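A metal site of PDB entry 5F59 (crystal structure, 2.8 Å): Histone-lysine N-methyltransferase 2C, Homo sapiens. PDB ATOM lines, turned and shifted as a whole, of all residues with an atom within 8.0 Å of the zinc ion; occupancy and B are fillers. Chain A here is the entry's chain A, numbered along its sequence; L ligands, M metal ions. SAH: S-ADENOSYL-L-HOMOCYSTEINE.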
ATOM      1  N   ILE A  24      11.813  10.150 -13.096  1.00  0.00           N
ATOM      2  CA  ILE A  24      12.697   9.951 -14.254  1.00  0.00           C
ATOM      3  C   ILE A  24      14.171  10.023 -13.870  1.00  0.00           C
ATOM      4  O   ILE A  24      14.906   9.058 -14.069  1.00  0.00           O
ATOM      5  CB  ILE A  24      12.373  10.974 -15.353  1.00  0.00           C
ATOM      6  CG1 ILE A  24      10.911  10.815 -15.780  1.00  0.00           C
ATOM      7  CG2 ILE A  24      13.330  10.795 -16.533  1.00  0.00           C
ATOM      8  CD1 ILE A  24      10.438  11.790 -16.832  1.00  0.00           C
ATOM      9  N   HIS A  93      13.570  15.210 -19.621  1.00  0.00           N
ATOM     10  CA  HIS A  93      13.233  14.769 -20.973  1.00  0.00           C
ATOM     11  C   HIS A  93      12.293  13.558 -20.975  1.00  0.00           C
ATOM     12  O   HIS A  93      12.435  12.661 -20.143  1.00  0.00           O
ATOM     13  CB  HIS A  93      14.496  14.419 -21.775  1.00  0.00           C
ATOM     14  CG  HIS A  93      14.225  13.543 -22.964  1.00  0.00           C
ATOM     15  ND1 HIS A  93      13.716  14.028 -24.153  1.00  0.00           N
ATOM     16  CD2 HIS A  93      14.355  12.202 -23.124  1.00  0.00           C
ATOM     17  CE1 HIS A  93      13.550  13.030 -24.993  1.00  0.00           C
ATOM     18  NE2 HIS A  93      13.927  11.906 -24.399  1.00  0.00           N
ATOM     19  N   SER A  94      11.370  13.526 -21.920  1.00  0.00           N
ATOM     20  CA  SER A  94      10.612  12.309 -22.142  1.00  0.00           C
ATOM     21  C   SER A  94      10.478  11.981 -23.614  1.00  0.00           C
ATOM     22  O   SER A  94      10.298  12.867 -24.456  1.00  0.00           O
ATOM     23  CB  SER A  94       9.224  12.403 -21.529  1.00  0.00           C
ATOM     24  OG  SER A  94       8.435  11.269 -21.872  1.00  0.00           O
ATOM     25  N   CYS A  95      10.547  10.685 -23.910  1.00  0.00           N
ATOM     26  CA  CYS A  95      10.242  10.184 -25.233  1.00  0.00           C
ATOM     27  C   CYS A  95       8.749  10.291 -25.522  1.00  0.00           C
ATOM     28  O   CYS A  95       8.337  10.272 -26.673  1.00  0.00           O
ATOM     29  CB  CYS A  95      10.706   8.749 -25.371  1.00  0.00           C
ATOM     30  SG  CYS A  95      12.492   8.631 -25.284  1.00  0.00           S
ATOM     31  N   ALA A  96       7.948  10.431 -24.463  1.00  0.00           N
ATOM     32  CA  ALA A  96       6.501  10.601 -24.589  1.00  0.00           C
ATOM     33  C   ALA A  96       6.035  11.783 -23.736  1.00  0.00           C
ATOM     34  O   ALA A  96       5.384  11.599 -22.710  1.00  0.00           O
ATOM     35  CB  ALA A  96       5.780   9.335 -24.180  1.00  0.00           C
ATOM     36  N   PHE A 132      17.334  15.276 -29.570  1.00  0.00           N
ATOM     37  CA  PHE A 132      18.782  15.026 -29.604  1.00  0.00           C
ATOM     38  C   PHE A 132      19.369  14.915 -31.014  1.00  0.00           C
ATOM     39  O   PHE A 132      18.683  14.555 -31.968  1.00  0.00           O
ATOM     40  CB  PHE A 132      19.107  13.745 -28.839  1.00  0.00           C
ATOM     41  CG  PHE A 132      18.731  13.803 -27.400  1.00  0.00           C
ATOM     42  CD1 PHE A 132      19.451  14.629 -26.535  1.00  0.00           C
ATOM     43  CD2 PHE A 132      17.673  13.044 -26.912  1.00  0.00           C
ATOM     44  CE1 PHE A 132      19.112  14.701 -25.204  1.00  0.00           C
ATOM     45  CE2 PHE A 132      17.326  13.096 -25.584  1.00  0.00           C
ATOM     46  CZ  PHE A 132      18.049  13.931 -24.722  1.00  0.00           C
ATOM     47  N   PRO A 142      21.736   6.543 -21.386  1.00  0.00           N
ATOM     48  CA  PRO A 142      20.409   5.901 -21.418  1.00  0.00           C
ATOM     49  C   PRO A 142      19.262   6.780 -20.911  1.00  0.00           C
ATOM     50  O   PRO A 142      19.362   7.462 -19.886  1.00  0.00           O
ATOM     51  CB  PRO A 142      20.581   4.682 -20.497  1.00  0.00           C
ATOM     52  CG  PRO A 142      21.721   5.040 -19.604  1.00  0.00           C
ATOM     53  CD  PRO A 142      22.642   5.851 -20.446  1.00  0.00           C
ATOM     54  N   CYS A 143      18.158   6.737 -21.653  1.00  0.00           N
ATOM     55  CA  CYS A 143      16.938   7.437 -21.283  1.00  0.00           C
ATOM     56  C   CYS A 143      16.154   6.658 -20.226  1.00  0.00           C
ATOM     57  O   CYS A 143      16.026   5.436 -20.317  1.00  0.00           O
ATOM     58  CB  CYS A 143      16.055   7.663 -22.507  1.00  0.00           C
ATOM     59  SG  CYS A 143      14.505   8.488 -22.137  1.00  0.00           S
ATOM     60  N   HIS A 144      15.637   7.373 -19.238  1.00  0.00           N
ATOM     61  CA  HIS A 144      14.854   6.785 -18.158  1.00  0.00           C
ATOM     62  C   HIS A 144      13.426   7.321 -18.100  1.00  0.00           C
ATOM     63  O   HIS A 144      12.804   7.318 -17.044  1.00  0.00           O
ATOM     64  CB  HIS A 144      15.507   7.025 -16.814  1.00  0.00           C
ATOM     65  CG  HIS A 144      16.744   6.215 -16.586  1.00  0.00           C
ATOM     66  ND1 HIS A 144      16.943   4.987 -17.175  1.00  0.00           N
ATOM     67  CD2 HIS A 144      17.846   6.447 -15.831  1.00  0.00           C
ATOM     68  CE1 HIS A 144      18.107   4.490 -16.791  1.00  0.00           C
ATOM     69  NE2 HIS A 144      18.676   5.360 -15.977  1.00  0.00           N
ATOM     70  N   CYS A 145      12.914   7.784 -19.229  1.00  0.00           N
ATOM     71  CA  CYS A 145      11.595   8.403 -19.228  1.00  0.00           C
ATOM     72  C   CYS A 145      10.511   7.351 -18.984  1.00  0.00           C
ATOM     73  O   CYS A 145       9.341   7.678 -18.738  1.00  0.00           O
ATOM     74  CB  CYS A 145      11.336   9.136 -20.551  1.00  0.00           C
ATOM     75  SG  CYS A 145      11.058   8.055 -21.970  1.00  0.00           S
ATOM     76  N   GLY A 146      10.901   6.080 -19.064  1.00  0.00           N
ATOM     77  CA  GLY A 146       9.984   4.967 -18.864  1.00  0.00           C
ATOM     78  C   GLY A 146       8.930   4.702 -19.939  1.00  0.00           C
ATOM     79  O   GLY A 146       8.177   3.755 -19.821  1.00  0.00           O
ATOM     80  N   ALA A 147       8.872   5.520 -20.992  1.00  0.00           N
ATOM     81  CA  ALA A 147       7.815   5.375 -21.992  1.00  0.00           C
ATOM     82  C   ALA A 147       7.927   4.071 -22.763  1.00  0.00           C
ATOM     83  O   ALA A 147       9.017   3.478 -22.856  1.00  0.00           O
ATOM     84  CB  ALA A 147       7.825   6.546 -22.964  1.00  0.00           C
ATOM     85  N   VAL A 148       6.800   3.632 -23.298  1.00  0.00           N
ATOM     86  CA  VAL A 148       6.763   2.427 -24.124  1.00  0.00           C
ATOM     87  C   VAL A 148       7.690   2.605 -25.329  1.00  0.00           C
ATOM     88  O   VAL A 148       8.547   1.759 -25.598  1.00  0.00           O
ATOM     89  CB  VAL A 148       5.325   2.114 -24.600  1.00  0.00           C
ATOM     90  CG1 VAL A 148       5.322   0.980 -25.601  1.00  0.00           C
ATOM     91  CG2 VAL A 148       4.430   1.767 -23.421  1.00  0.00           C
ATOM     92  N   ASN A 149       7.539   3.721 -26.037  1.00  0.00           N
ATOM     93  CA  ASN A 149       8.322   3.970 -27.238  1.00  0.00           C
ATOM     94  C   ASN A 149       9.586   4.804 -26.966  1.00  0.00           C
ATOM     95  O   ASN A 149       9.997   5.647 -27.763  1.00  0.00           O
ATOM     96  CB  ASN A 149       7.443   4.649 -28.276  1.00  0.00           C
ATOM     97  CG  ASN A 149       6.264   3.770 -28.703  1.00  0.00           C
ATOM     98  OD1 ASN A 149       6.328   2.543 -28.624  1.00  0.00           O
ATOM     99  ND2 ASN A 149       5.186   4.401 -29.154  1.00  0.00           N
ATOM    100  N   CYS A 150      10.208   4.532 -25.818  1.00  0.00           N
ATOM    101  CA  CYS A 150      11.449   5.165 -25.435  1.00  0.00           C
ATOM    102  C   CYS A 150      12.536   4.872 -26.466  1.00  0.00           C
ATOM    103  O   CYS A 150      12.641   3.753 -26.955  1.00  0.00           O
ATOM    104  CB  CYS A 150      11.878   4.677 -24.057  1.00  0.00           C
ATOM    105  SG  CYS A 150      13.359   5.426 -23.368  1.00  0.00           S
ATOM    106  N   ARG A 151      13.337   5.881 -26.803  1.00  0.00           N
ATOM    107  CA  ARG A 151      14.434   5.709 -27.741  1.00  0.00           C
ATOM    108  C   ARG A 151      15.686   5.205 -27.026  1.00  0.00           C
ATOM    109  O   ARG A 151      16.783   5.256 -27.568  1.00  0.00           O
ATOM    110  CB  ARG A 151      14.756   7.019 -28.451  1.00  0.00           C
ATOM    111  CG  ARG A 151      13.530   7.769 -28.930  1.00  0.00           C
ATOM    112  CD  ARG A 151      13.947   8.976 -29.751  1.00  0.00           C
ATOM    113  NE  ARG A 151      12.931  10.018 -29.720  1.00  0.00           N
ATOM    114  CZ  ARG A 151      13.056  11.173 -29.092  1.00  0.00           C
ATOM    115  NH1 ARG A 151      14.176  11.472 -28.444  1.00  0.00           N
ATOM    116  NH2 ARG A 151      12.056  12.047 -29.127  1.00  0.00           N
ATOM    117  N   LYS A 152      15.512   4.756 -25.785  1.00  0.00           N
ATOM    118  CA  LYS A 152      16.578   4.162 -24.992  1.00  0.00           C
ATOM    119  C   LYS A 152      17.758   5.093 -24.674  1.00  0.00           C
ATOM    120  O   LYS A 152      18.362   4.952 -23.620  1.00  0.00           O
ATOM    121  CB  LYS A 152      17.098   2.891 -25.685  1.00  0.00           C
ATOM    122  N   TRP A 153      18.095   6.038 -25.555  1.00  0.00           N
ATOM    123  CA  TRP A 153      19.254   6.916 -25.314  1.00  0.00           C
ATOM    124  C   TRP A 153      18.983   8.433 -25.454  1.00  0.00           C
ATOM    125  O   TRP A 153      18.040   8.872 -26.096  1.00  0.00           O
ATOM    126  CB  TRP A 153      20.398   6.535 -26.271  1.00  0.00           C
ATOM    127  CG  TRP A 153      20.683   5.070 -26.317  1.00  0.00           C
ATOM    128  CD1 TRP A 153      20.199   4.165 -27.226  1.00  0.00           C
ATOM    129  CD2 TRP A 153      21.502   4.337 -25.399  1.00  0.00           C
ATOM    130  NE1 TRP A 153      20.670   2.908 -26.926  1.00  0.00           N
ATOM    131  CE2 TRP A 153      21.468   2.986 -25.805  1.00  0.00           C
ATOM    132  CE3 TRP A 153      22.247   4.689 -24.275  1.00  0.00           C
ATOM    133  CZ2 TRP A 153      22.174   1.985 -25.128  1.00  0.00           C
ATOM    134  CZ3 TRP A 153      22.944   3.692 -23.597  1.00  0.00           C
ATOM    135  CH2 TRP A 153      22.892   2.359 -24.036  1.00  0.00           C
ATOM    136  N   MET A 154      19.859   9.224 -24.828  1.00  0.00           N
ATOM    137  CA  MET A 154      19.821  10.672 -24.961  1.00  0.00           C
ATOM    138  C   MET A 154      21.017  11.222 -25.744  1.00  0.00           C
ATOM    139  O   MET A 154      22.151  11.245 -25.248  1.00  0.00           O
ATOM    140  CB  MET A 154      19.764  11.307 -23.580  1.00  0.00           C
ATOM    141  CG  MET A 154      18.475  11.076 -22.840  1.00  0.00           C
ATOM    142  SD  MET A 154      18.369  12.243 -21.462  1.00  0.00           S
ATOM    143  CE  MET A 154      19.680  11.626 -20.454  1.00  0.00           C
HETATM  144  N   SAH L   1      16.647  15.747 -13.507  1.00  0.00           N
HETATM  145  CA  SAH L   1      17.471  16.955 -13.552  1.00  0.00           C
HETATM  146  CB  SAH L   1      16.711  18.168 -14.082  1.00  0.00           C
HETATM  147  CG  SAH L   1      16.854  18.394 -15.596  1.00  0.00           C
HETATM  148  SD  SAH L   1      18.549  18.871 -16.050  1.00  0.00           S
HETATM  149  C   SAH L   1      18.052  17.224 -12.178  1.00  0.00           C
HETATM  150  O   SAH L   1      18.840  18.150 -12.002  1.00  0.00           O
HETATM  151  OXT SAH L   1      17.759  16.506 -11.219  1.00  0.00           O
HETATM  152  C5' SAH L   1      18.657  17.682 -17.422  1.00  0.00           C
HETATM  153  C4' SAH L   1      19.492  16.487 -16.978  1.00  0.00           C
HETATM  154  O4' SAH L   1      18.655  15.579 -16.278  1.00  0.00           O
HETATM  155  C3' SAH L   1      20.161  15.727 -18.107  1.00  0.00           C
HETATM  156  O3' SAH L   1      21.492  16.139 -18.300  1.00  0.00           O
HETATM  157  C2' SAH L   1      20.129  14.305 -17.603  1.00  0.00           C
HETATM  158  O2' SAH L   1      21.241  14.030 -16.790  1.00  0.00           O
HETATM  159  C1' SAH L   1      18.917  14.251 -16.695  1.00  0.00           C
HETATM  160  N9  SAH L   1      17.744  13.735 -17.432  1.00  0.00           N
HETATM  161  C8  SAH L   1      16.694  14.478 -17.887  1.00  0.00           C
HETATM  162  N7  SAH L   1      15.818  13.664 -18.518  1.00  0.00           N
HETATM  163  C5  SAH L   1      16.303  12.400 -18.473  1.00  0.00           C
HETATM  164  C6  SAH L   1      15.810  11.199 -18.951  1.00  0.00           C
HETATM  165  N6  SAH L   1      14.649  11.153 -19.604  1.00  0.00           N
HETATM  166  N1  SAH L   1      16.538  10.048 -18.759  1.00  0.00           N
HETATM  167  C2  SAH L   1      17.733  10.089 -18.080  1.00  0.00           C
HETATM  168  N3  SAH L   1      18.224  11.288 -17.611  1.00  0.00           N
HETATM  169  C4  SAH L   1      17.516  12.433 -17.796  1.00  0.00           C
HETATM  170 ZN    ZN M   1      12.925   7.814 -23.332  1.00  0.00          ZN
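The side-chain sulfur of Cys 143 sits close to a nitrogen (N6) of the ligand, at 3.7 Å.
The backbone NH (N) of His 93 lies within hydrogen-bond range of a nitrogen (N7) of the ligand (2.9 Å).
O of His 93 sits at hydrogen-bond distance from N6 of the ligand (2.7 Å).
A nitrogen (N1) of the ligand lies within hydrogen-bond range of the backbone NH (N) of His 144 (2.9 Å).
N of Cys 143 lies within hydrogen-bond range of O of Lys 152 (2.7 Å).
The side-chain sulfur (SG) of Cys 95 lies close to the backbone NH (N) of Arg 151 (3.3 Å).
A ring nitrogen (NE2) of His 93 lies close to the side-chain sulfur of Cys 95 (3.7 Å).
The side-chain sulfur of Cys 145 sits close to the backbone NH of Ala 147, 3.5 Å away.
The side-chain sulfur (SG) of Cys 150 lies close to the backbone NH (N) of Lys 152 (3.3 Å).
Merely in contact with the zinc ion: Arg 151.
Five residues have an atom within 4 Å of the zinc ion: Cys 95, Cys 143, Cys 145, Cys 150 and Arg 151.
The zinc ion is bound by SG of Cys 143.
The zinc ion is bound by SG of Cys 95 (2.2 Å).
SG of Cys 145 binds the zinc ion, at 2.3 Å.
SG of Cys 150 binds the zinc ion (2.4 Å).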
